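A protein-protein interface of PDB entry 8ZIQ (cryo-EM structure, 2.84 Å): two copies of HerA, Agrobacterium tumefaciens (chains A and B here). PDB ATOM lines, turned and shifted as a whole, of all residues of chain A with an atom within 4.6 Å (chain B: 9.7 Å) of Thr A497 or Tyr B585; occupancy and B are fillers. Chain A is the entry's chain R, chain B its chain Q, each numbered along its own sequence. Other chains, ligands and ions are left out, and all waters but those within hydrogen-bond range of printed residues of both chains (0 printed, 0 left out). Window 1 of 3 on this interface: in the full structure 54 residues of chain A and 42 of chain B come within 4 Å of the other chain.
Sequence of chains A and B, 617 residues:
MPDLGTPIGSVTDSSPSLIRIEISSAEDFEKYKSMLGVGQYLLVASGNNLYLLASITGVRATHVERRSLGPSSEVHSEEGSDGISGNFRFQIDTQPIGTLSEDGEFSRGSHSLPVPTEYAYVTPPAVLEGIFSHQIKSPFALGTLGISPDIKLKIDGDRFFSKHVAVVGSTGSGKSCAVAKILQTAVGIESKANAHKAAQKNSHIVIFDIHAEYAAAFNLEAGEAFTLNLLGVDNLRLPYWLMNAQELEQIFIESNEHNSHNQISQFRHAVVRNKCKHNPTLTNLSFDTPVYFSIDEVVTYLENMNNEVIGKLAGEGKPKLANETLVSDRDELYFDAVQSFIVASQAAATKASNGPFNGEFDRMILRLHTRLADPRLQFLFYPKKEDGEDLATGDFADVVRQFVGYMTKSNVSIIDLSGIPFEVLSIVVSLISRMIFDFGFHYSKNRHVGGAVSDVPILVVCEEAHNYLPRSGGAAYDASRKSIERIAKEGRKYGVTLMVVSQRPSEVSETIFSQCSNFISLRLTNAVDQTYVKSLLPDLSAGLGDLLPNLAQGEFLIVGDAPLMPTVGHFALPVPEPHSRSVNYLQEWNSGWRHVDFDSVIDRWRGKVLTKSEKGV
Printed residues of chain B that touch a printed residue of chain A: Ser B582, Val B583, Asn B584, Tyr B585, Leu B586 and Trp B589. Hydrophobic or aromatic side chains of chain B within 4 Å of the printed part of chain A: Val B583, Tyr B585, Leu B586 and Trp B589. Printed residues of chain A that touch a printed residue of chain B: Asp A158, Phe A161, Ser A162, Pro A457, Arg A492, Gly A495, Val A496 and Thr A497. Hydrophobic or aromatic side chains of chain A that line the printed part of chain B: Phe A161 and Pro A457.
The backbone carbonyl oxygen (O) of Leu B586 sits at hydrogen-bond distance from the side-chain amide nitrogen (ND2) of Asn B590, at 2.9 Å. O of Ile A458 lies within hydrogen-bond range of N of Thr A497 (3.0 Å). The side-chain hydroxyl (OG) of Ser A162 lies within hydrogen-bond range of the backbone carbonyl oxygen (O) of Asp A158, at 2.8 Å. The side-chain amide oxygen (OD1) of Asn B584 sits close to the side-chain amide oxygen (OE1) of Gln B587 (3.3 Å). The backbone NH (N) of Ile A458 lies within hydrogen-bond range of the backbone carbonyl oxygen (O) of Gly A495, at 3.0 Å. The backbone NH (N) of Val A460 is in hydrogen-bond range of the backbone carbonyl oxygen (O) of Thr A497 (2.9 Å).
The backbone NH of Tyr B585 lies within hydrogen-bond range of the side-chain carboxylate of Asp A158, 3.5 Å away. OH of Tyr B585 sits at hydrogen-bond distance from O of Gly A495. The side-chain hydroxyl (OG) of Ser A162 sits at hydrogen-bond distance from the backbone carbonyl oxygen (O) of Val B583, at 3.4 Å.
No position is printed for both chains.
Asp A158 touches Asn B584 (OD1 to CB, 3.4 Å). Leu B586 touches Asp A158. O of Phe A161 touches CD2 of Tyr B585, at 3.2 Å. CD2 of Leu B586 touches CD2 of Phe A161, at 3.6 Å. CD1 of Tyr B585 touches CB of Pro A457, 3.7 Å away. CG of Pro A457 touches NE1 of Trp B589, at 3.4 Å. OG of Ser B582 touches NH2 of Arg A492, at 3.8 Å. Val B583 touches Arg A492 (CG1 to O, 3.3 Å). Val A496 touches Tyr B585 (N to OH, 3.8 Å). CG2 of Thr A497 touches CE2 of Tyr B585 (3.2 Å).
Of chain B, only Val B583 (3.4 Å) comes within 4 Å of Ser A162. Of the printed residues of chain B, Pro A457 touches Tyr B585 (3.7 Å) and Trp B589 (3.4 Å). Ile A458 touches none of the printed residues of chain B. No residue of chain B comes within 4 Å of Leu A459. No residue of chain B comes within 4 Å of Val A460. Of chain B, only Tyr B585 comes within 4 Å of Gly A495. Val A496 touches just one residue of chain B: Tyr B585 (3.8 Å). Thr A497 touches just one residue of chain B: Tyr B585. Of the printed residues of chain A, Ser B582 touches Arg A492 (3.8 Å). Printed residues of chain A within 4 Å of Val B583: Ser A162 (3.4 Å) and Arg A492 (3.3 Å). Of the printed residues of chain A, Asn B584 touches Asp A158 (3.4 Å). Tyr B585 touches just these residues of chain A: Asp A158, Phe A161, Pro A457, Gly A495, Val A496 and Thr A497. Of the printed residues of chain A, Leu B586 touches Asp A158 and Phe A161. Ser B591 touches none of the printed residues of chain A. The nearest printed residue of chain B that does not touch Pro A457 is Glu B588 (4.4 Å).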
ATOM      1  N   ASP A 158      -4.442  22.686   0.616  1.00  0.00           N
ATOM      2  CA  ASP A 158      -5.139  21.575  -0.003  1.00  0.00           C
ATOM      3  C   ASP A 158      -5.648  20.611   1.054  1.00  0.00           C
ATOM      4  O   ASP A 158      -6.847  20.332   1.134  1.00  0.00           O
ATOM      5  CB  ASP A 158      -4.207  20.869  -0.979  1.00  0.00           C
ATOM      6  CG  ASP A 158      -4.040  21.632  -2.275  1.00  0.00           C
ATOM      7  OD1 ASP A 158      -5.009  22.278  -2.718  1.00  0.00           O
ATOM      8  OD2 ASP A 158      -2.936  21.581  -2.855  1.00  0.00           O
ATOM      9  N   PHE A 161      -8.748  22.029   2.675  1.00  0.00           N
ATOM     10  CA  PHE A 161      -9.989  22.035   1.912  1.00  0.00           C
ATOM     11  C   PHE A 161     -10.222  20.763   1.114  1.00  0.00           C
ATOM     12  O   PHE A 161     -11.360  20.510   0.707  1.00  0.00           O
ATOM     13  CB  PHE A 161     -10.010  23.234   0.960  1.00  0.00           C
ATOM     14  CG  PHE A 161     -10.433  24.523   1.599  1.00  0.00           C
ATOM     15  CD1 PHE A 161     -11.400  24.558   2.580  1.00  0.00           C
ATOM     16  CD2 PHE A 161      -9.861  25.707   1.210  1.00  0.00           C
ATOM     17  CE1 PHE A 161     -11.772  25.743   3.147  1.00  0.00           C
ATOM     18  CE2 PHE A 161     -10.237  26.883   1.781  1.00  0.00           C
ATOM     19  CZ  PHE A 161     -11.189  26.899   2.748  1.00  0.00           C
ATOM     20  N   SER A 162      -9.192  19.952   0.889  1.00  0.00           N
ATOM     21  CA  SER A 162      -9.376  18.692   0.188  1.00  0.00           C
ATOM     22  C   SER A 162     -10.036  17.640   1.054  1.00  0.00           C
ATOM     23  O   SER A 162     -10.351  16.558   0.553  1.00  0.00           O
ATOM     24  CB  SER A 162      -8.046  18.165  -0.329  1.00  0.00           C
ATOM     25  OG  SER A 162      -7.498  19.052  -1.288  1.00  0.00           O
ATOM     26  N   HIS A 164     -12.486  17.029   5.007  1.00  0.00           N
ATOM     27  CA  HIS A 164     -13.574  17.595   5.772  1.00  0.00           C
ATOM     28  C   HIS A 164     -13.060  18.251   7.043  1.00  0.00           C
ATOM     29  O   HIS A 164     -12.178  17.725   7.725  1.00  0.00           O
ATOM     30  CB  HIS A 164     -14.600  16.511   6.080  1.00  0.00           C
ATOM     31  CG  HIS A 164     -15.138  15.838   4.859  1.00  0.00           C
ATOM     32  ND1 HIS A 164     -16.099  16.409   4.058  1.00  0.00           N
ATOM     33  CD2 HIS A 164     -14.855  14.639   4.303  1.00  0.00           C
ATOM     34  CE1 HIS A 164     -16.379  15.596   3.059  1.00  0.00           C
ATOM     35  NE2 HIS A 164     -15.639  14.512   3.186  1.00  0.00           N
ATOM     36  N   PRO A 457     -14.704  22.482  -8.285  1.00  0.00           N
ATOM     37  CA  PRO A 457     -14.810  22.036  -6.897  1.00  0.00           C
ATOM     38  C   PRO A 457     -15.889  22.753  -6.114  1.00  0.00           C
ATOM     39  O   PRO A 457     -15.922  23.984  -6.085  1.00  0.00           O
ATOM     40  CB  PRO A 457     -13.426  22.340  -6.353  1.00  0.00           C
ATOM     41  CG  PRO A 457     -13.016  23.494  -7.091  1.00  0.00           C
ATOM     42  CD  PRO A 457     -13.521  23.321  -8.471  1.00  0.00           C
ATOM     43  N   ILE A 458     -16.760  21.998  -5.462  1.00  0.00           N
ATOM     44  CA  ILE A 458     -17.836  22.558  -4.665  1.00  0.00           C
ATOM     45  C   ILE A 458     -17.620  22.276  -3.191  1.00  0.00           C
ATOM     46  O   ILE A 458     -17.143  21.204  -2.788  1.00  0.00           O
ATOM     47  CB  ILE A 458     -19.202  22.014  -5.108  1.00  0.00           C
ATOM     48  CG1 ILE A 458     -19.491  22.390  -6.554  1.00  0.00           C
ATOM     49  CG2 ILE A 458     -20.284  22.546  -4.224  1.00  0.00           C
ATOM     50  CD1 ILE A 458     -19.108  21.330  -7.540  1.00  0.00           C
ATOM     51  N   LEU A 459     -18.042  23.234  -2.374  1.00  0.00           N
ATOM     52  CA  LEU A 459     -17.972  23.079  -0.935  1.00  0.00           C
ATOM     53  C   LEU A 459     -19.293  23.483  -0.307  1.00  0.00           C
ATOM     54  O   LEU A 459     -19.806  24.576  -0.565  1.00  0.00           O
ATOM     55  CB  LEU A 459     -16.853  23.923  -0.361  1.00  0.00           C
ATOM     56  CG  LEU A 459     -16.938  24.255   1.112  1.00  0.00           C
ATOM     57  CD1 LEU A 459     -16.978  23.008   1.984  1.00  0.00           C
ATOM     58  CD2 LEU A 459     -15.781  25.106   1.461  1.00  0.00           C
ATOM     59  N   VAL A 460     -19.817  22.598   0.528  1.00  0.00           N
ATOM     60  CA  VAL A 460     -21.049  22.797   1.267  1.00  0.00           C
ATOM     61  C   VAL A 460     -20.672  23.165   2.687  1.00  0.00           C
ATOM     62  O   VAL A 460     -19.860  22.479   3.318  1.00  0.00           O
ATOM     63  CB  VAL A 460     -21.928  21.542   1.241  1.00  0.00           C
ATOM     64  CG1 VAL A 460     -23.197  21.785   1.986  1.00  0.00           C
ATOM     65  CG2 VAL A 460     -22.229  21.143  -0.150  1.00  0.00           C
ATOM     66  N   ARG A 492     -14.471  13.248  -1.567  1.00  0.00           N
ATOM     67  CA  ARG A 492     -13.213  13.826  -2.013  1.00  0.00           C
ATOM     68  C   ARG A 492     -12.915  13.454  -3.450  1.00  0.00           C
ATOM     69  O   ARG A 492     -12.297  14.234  -4.181  1.00  0.00           O
ATOM     70  CB  ARG A 492     -12.080  13.381  -1.103  1.00  0.00           C
ATOM     71  CG  ARG A 492     -12.256  13.800   0.336  1.00  0.00           C
ATOM     72  CD  ARG A 492     -11.099  13.297   1.156  1.00  0.00           C
ATOM     73  NE  ARG A 492      -9.846  13.863   0.666  1.00  0.00           N
ATOM     74  CZ  ARG A 492      -8.850  13.160   0.137  1.00  0.00           C
ATOM     75  NH1 ARG A 492      -8.923  11.840   0.041  1.00  0.00           N
ATOM     76  NH2 ARG A 492      -7.758  13.784  -0.281  1.00  0.00           N
ATOM     77  N   GLY A 495     -15.405  15.684  -6.037  1.00  0.00           N
ATOM     78  CA  GLY A 495     -15.365  17.122  -6.111  1.00  0.00           C
ATOM     79  C   GLY A 495     -16.069  17.889  -5.019  1.00  0.00           C
ATOM     80  O   GLY A 495     -15.939  19.113  -4.951  1.00  0.00           O
ATOM     81  N   VAL A 496     -16.796  17.204  -4.149  1.00  0.00           N
ATOM     82  CA  VAL A 496     -17.676  17.841  -3.183  1.00  0.00           C
ATOM     83  C   VAL A 496     -17.102  17.643  -1.797  1.00  0.00           C
ATOM     84  O   VAL A 496     -16.743  16.522  -1.421  1.00  0.00           O
ATOM     85  CB  VAL A 496     -19.094  17.271  -3.253  1.00  0.00           C
ATOM     86  CG1 VAL A 496     -19.941  17.880  -2.194  1.00  0.00           C
ATOM     87  CG2 VAL A 496     -19.677  17.514  -4.577  1.00  0.00           C
ATOM     88  N   THR A 497     -17.023  18.726  -1.035  1.00  0.00           N
ATOM     89  CA  THR A 497     -16.574  18.653   0.344  1.00  0.00           C
ATOM     90  C   THR A 497     -17.540  19.355   1.282  1.00  0.00           C
ATOM     91  O   THR A 497     -18.419  20.109   0.863  1.00  0.00           O
ATOM     92  CB  THR A 497     -15.181  19.240   0.501  1.00  0.00           C
ATOM     93  OG1 THR A 497     -15.157  20.584   0.009  1.00  0.00           O
ATOM     94  CG2 THR A 497     -14.224  18.399  -0.242  1.00  0.00           C
ATOM     95  N   LEU A 498     -17.360  19.077   2.570  1.00  0.00           N
ATOM     96  CA  LEU A 498     -18.298  19.449   3.613  1.00  0.00           C
ATOM     97  C   LEU A 498     -17.591  20.127   4.775  1.00  0.00           C
ATOM     98  O   LEU A 498     -16.472  19.759   5.134  1.00  0.00           O
ATOM     99  CB  LEU A 498     -19.015  18.231   4.114  1.00  0.00           C
ATOM    100  CG  LEU A 498     -20.297  18.412   4.891  1.00  0.00           C
ATOM    101  CD1 LEU A 498     -21.141  17.217   4.617  1.00  0.00           C
ATOM    102  CD2 LEU A 498     -20.038  18.549   6.367  1.00  0.00           C
ATOM    103  N   MET A 499     -18.249  21.133   5.348  1.00  0.00           N
ATOM    104  CA  MET A 499     -17.778  21.826   6.543  1.00  0.00           C
ATOM    105  C   MET A 499     -18.938  21.980   7.510  1.00  0.00           C
ATOM    106  O   MET A 499     -19.957  22.587   7.163  1.00  0.00           O
ATOM    107  CB  MET A 499     -17.208  23.202   6.213  1.00  0.00           C
ATOM    108  CG  MET A 499     -16.756  23.971   7.427  1.00  0.00           C
ATOM    109  SD  MET A 499     -16.813  25.743   7.209  1.00  0.00           S
ATOM    110  CE  MET A 499     -15.149  26.007   6.687  1.00  0.00           C
ATOM    111  N   ARG B 581      -4.414  10.154  -7.568  1.00  0.00           N
ATOM    112  CA  ARG B 581      -4.931  11.228  -8.409  1.00  0.00           C
ATOM    113  C   ARG B 581      -5.995  12.003  -7.630  1.00  0.00           C
ATOM    114  O   ARG B 581      -7.188  11.987  -7.938  1.00  0.00           O
ATOM    115  CB  ARG B 581      -5.444  10.705  -9.739  1.00  0.00           C
ATOM    116  CG  ARG B 581      -5.421  11.820 -10.763  1.00  0.00           C
ATOM    117  CD  ARG B 581      -5.936  11.451 -12.127  1.00  0.00           C
ATOM    118  NE  ARG B 581      -5.769  12.606 -13.002  1.00  0.00           N
ATOM    119  CZ  ARG B 581      -6.012  12.609 -14.306  1.00  0.00           C
ATOM    120  NH1 ARG B 581      -6.442  11.510 -14.907  1.00  0.00           N
ATOM    121  NH2 ARG B 581      -5.806  13.714 -15.009  1.00  0.00           N
ATOM    122  N   SER B 582      -5.536  12.695  -6.597  1.00  0.00           N
ATOM    123  CA  SER B 582      -6.448  13.491  -5.800  1.00  0.00           C
ATOM    124  C   SER B 582      -6.654  14.840  -6.475  1.00  0.00           C
ATOM    125  O   SER B 582      -5.871  15.262  -7.329  1.00  0.00           O
ATOM    126  CB  SER B 582      -5.907  13.675  -4.381  1.00  0.00           C
ATOM    127  OG  SER B 582      -6.521  14.777  -3.735  1.00  0.00           O
ATOM    128  N   VAL B 583      -7.710  15.532  -6.067  1.00  0.00           N
ATOM    129  CA  VAL B 583      -8.046  16.841  -6.610  1.00  0.00           C
ATOM    130  C   VAL B 583      -7.712  17.914  -5.591  1.00  0.00           C
ATOM    131  O   VAL B 583      -8.104  17.829  -4.421  1.00  0.00           O
ATOM    132  CB  VAL B 583      -9.527  16.898  -7.036  1.00  0.00           C
ATOM    133  CG1 VAL B 583     -10.388  16.128  -6.081  1.00  0.00           C
ATOM    134  CG2 VAL B 583     -10.037  18.334  -7.089  1.00  0.00           C
ATOM    135  N   ASN B 584      -6.984  18.924  -6.055  1.00  0.00           N
ATOM    136  CA  ASN B 584      -6.586  20.068  -5.258  1.00  0.00           C
ATOM    137  C   ASN B 584      -7.550  21.219  -5.510  1.00  0.00           C
ATOM    138  O   ASN B 584      -7.865  21.521  -6.665  1.00  0.00           O
ATOM    139  CB  ASN B 584      -5.159  20.476  -5.623  1.00  0.00           C
ATOM    140  CG  ASN B 584      -4.231  19.279  -5.780  1.00  0.00           C
ATOM    141  OD1 ASN B 584      -3.884  18.896  -6.898  1.00  0.00           O
ATOM    142  ND2 ASN B 584      -3.798  18.705  -4.662  1.00  0.00           N
ATOM    143  N   TYR B 585      -8.011  21.863  -4.440  1.00  0.00           N
ATOM    144  CA  TYR B 585      -9.093  22.834  -4.565  1.00  0.00           C
ATOM    145  C   TYR B 585      -8.577  24.254  -4.774  1.00  0.00           C
ATOM    146  O   TYR B 585      -8.962  24.921  -5.739  1.00  0.00           O
ATOM    147  CB  TYR B 585     -10.069  22.780  -3.386  1.00  0.00           C
ATOM    148  CG  TYR B 585     -10.899  21.526  -3.341  1.00  0.00           C
ATOM    149  CD1 TYR B 585     -10.808  20.574  -4.342  1.00  0.00           C
ATOM    150  CD2 TYR B 585     -11.847  21.343  -2.362  1.00  0.00           C
ATOM    151  CE1 TYR B 585     -11.572  19.443  -4.315  1.00  0.00           C
ATOM    152  CE2 TYR B 585     -12.616  20.216  -2.327  1.00  0.00           C
ATOM    153  CZ  TYR B 585     -12.483  19.268  -3.315  1.00  0.00           C
ATOM    154  OH  TYR B 585     -13.246  18.124  -3.319  1.00  0.00           O
ATOM    155  N   LEU B 586      -7.721  24.737  -3.875  1.00  0.00           N
ATOM    156  CA  LEU B 586      -7.247  26.107  -3.991  1.00  0.00           C
ATOM    157  C   LEU B 586      -6.283  26.292  -5.149  1.00  0.00           C
ATOM    158  O   LEU B 586      -5.986  27.434  -5.509  1.00  0.00           O
ATOM    159  CB  LEU B 586      -6.558  26.532  -2.695  1.00  0.00           C
ATOM    160  CG  LEU B 586      -7.394  26.570  -1.422  1.00  0.00           C
ATOM    161  CD1 LEU B 586      -6.511  26.886  -0.235  1.00  0.00           C
ATOM    162  CD2 LEU B 586      -8.493  27.583  -1.542  1.00  0.00           C
ATOM    163  N   GLN B 587      -5.790  25.207  -5.734  1.00  0.00           N
ATOM    164  CA  GLN B 587      -4.999  25.331  -6.945  1.00  0.00           C
ATOM    165  C   GLN B 587      -5.898  25.547  -8.152  1.00  0.00           C
ATOM    166  O   GLN B 587      -5.468  26.137  -9.149  1.00  0.00           O
ATOM    167  CB  GLN B 587      -4.148  24.080  -7.134  1.00  0.00           C
ATOM    168  CG  GLN B 587      -3.076  24.183  -8.197  1.00  0.00           C
ATOM    169  CD  GLN B 587      -2.453  22.833  -8.507  1.00  0.00           C
ATOM    170  OE1 GLN B 587      -2.682  21.857  -7.791  1.00  0.00           O
ATOM    171  NE2 GLN B 587      -1.665  22.769  -9.573  1.00  0.00           N
ATOM    172  N   GLU B 588      -7.142  25.074  -8.073  1.00  0.00           N
ATOM    173  CA  GLU B 588      -8.128  25.256  -9.128  1.00  0.00           C
ATOM    174  C   GLU B 588      -8.916  26.549  -8.997  1.00  0.00           C
ATOM    175  O   GLU B 588      -9.270  27.155 -10.015  1.00  0.00           O
ATOM    176  CB  GLU B 588      -9.117  24.094  -9.122  1.00  0.00           C
ATOM    177  CG  GLU B 588      -8.719  22.901  -9.951  1.00  0.00           C
ATOM    178  CD  GLU B 588      -8.600  23.212 -11.428  1.00  0.00           C
ATOM    179  OE1 GLU B 588      -8.864  24.367 -11.820  1.00  0.00           O
ATOM    180  OE2 GLU B 588      -8.240  22.298 -12.200  1.00  0.00           O
ATOM    181  N   TRP B 589      -9.203  26.984  -7.770  1.00  0.00           N
ATOM    182  CA  TRP B 589      -9.863  28.269  -7.581  1.00  0.00           C
ATOM    183  C   TRP B 589      -9.069  29.414  -8.188  1.00  0.00           C
ATOM    184  O   TRP B 589      -9.646  30.324  -8.792  1.00  0.00           O
ATOM    185  CB  TRP B 589     -10.094  28.541  -6.096  1.00  0.00           C
ATOM    186  CG  TRP B 589     -11.138  27.697  -5.422  1.00  0.00           C
ATOM    187  CD1 TRP B 589     -11.887  26.700  -5.970  1.00  0.00           C
ATOM    188  CD2 TRP B 589     -11.565  27.814  -4.066  1.00  0.00           C
ATOM    189  NE1 TRP B 589     -12.744  26.182  -5.034  1.00  0.00           N
ATOM    190  CE2 TRP B 589     -12.564  26.849  -3.855  1.00  0.00           C
ATOM    191  CE3 TRP B 589     -11.189  28.636  -3.005  1.00  0.00           C
ATOM    192  CZ2 TRP B 589     -13.187  26.683  -2.634  1.00  0.00           C
ATOM    193  CZ3 TRP B 589     -11.809  28.471  -1.796  1.00  0.00           C
ATOM    194  CH2 TRP B 589     -12.800  27.503  -1.616  1.00  0.00           C
ATOM    195  N   ASN B 590      -7.748  29.395  -8.033  1.00  0.00           N
ATOM    196  CA  ASN B 590      -6.922  30.447  -8.610  1.00  0.00           C
ATOM    197  C   ASN B 590      -7.221  30.639 -10.089  1.00  0.00           C
ATOM    198  O   ASN B 590      -7.172  31.762 -10.601  1.00  0.00           O
ATOM    199  CB  ASN B 590      -5.448  30.138  -8.373  1.00  0.00           C
ATOM    200  CG  ASN B 590      -5.022  30.441  -6.949  1.00  0.00           C
ATOM    201  OD1 ASN B 590      -5.412  31.462  -6.382  1.00  0.00           O
ATOM    202  ND2 ASN B 590      -4.226  29.557  -6.363  1.00  0.00           N
ATOM    203  N   SER B 591      -7.497  29.555 -10.798  1.00  0.00           N
ATOM    204  CA  SER B 591      -7.872  29.658 -12.196  1.00  0.00           C
ATOM    205  C   SER B 591      -9.222  30.358 -12.312  1.00  0.00           C
ATOM    206  O   SER B 591      -9.969  30.485 -11.340  1.00  0.00           O
ATOM    207  CB  SER B 591      -7.926  28.275 -12.847  1.00  0.00           C
ATOM    208  OG  SER B 591      -8.953  27.478 -12.285  1.00  0.00           O
ATOM    209  N   ARG B 594     -14.940  28.567 -15.612  1.00  0.00           N
ATOM    210  CA  ARG B 594     -14.902  27.563 -16.663  1.00  0.00           C
ATOM    211  C   ARG B 594     -16.329  27.298 -17.102  1.00  0.00           C
ATOM    212  O   ARG B 594     -17.164  26.910 -16.282  1.00  0.00           O
ATOM    213  CB  ARG B 594     -14.250  26.271 -16.170  1.00  0.00           C
ATOM    214  CG  ARG B 594     -12.756  26.381 -15.948  1.00  0.00           C
ATOM    215  CD  ARG B 594     -12.147  25.044 -15.584  1.00  0.00           C
ATOM    216  NE  ARG B 594     -10.737  25.160 -15.222  1.00  0.00           N
ATOM    217  CZ  ARG B 594      -9.718  25.072 -16.073  1.00  0.00           C
ATOM    218  NH1 ARG B 594      -9.928  24.855 -17.364  1.00  0.00           N
ATOM    219  NH2 ARG B 594      -8.477  25.193 -15.622  1.00  0.00           N
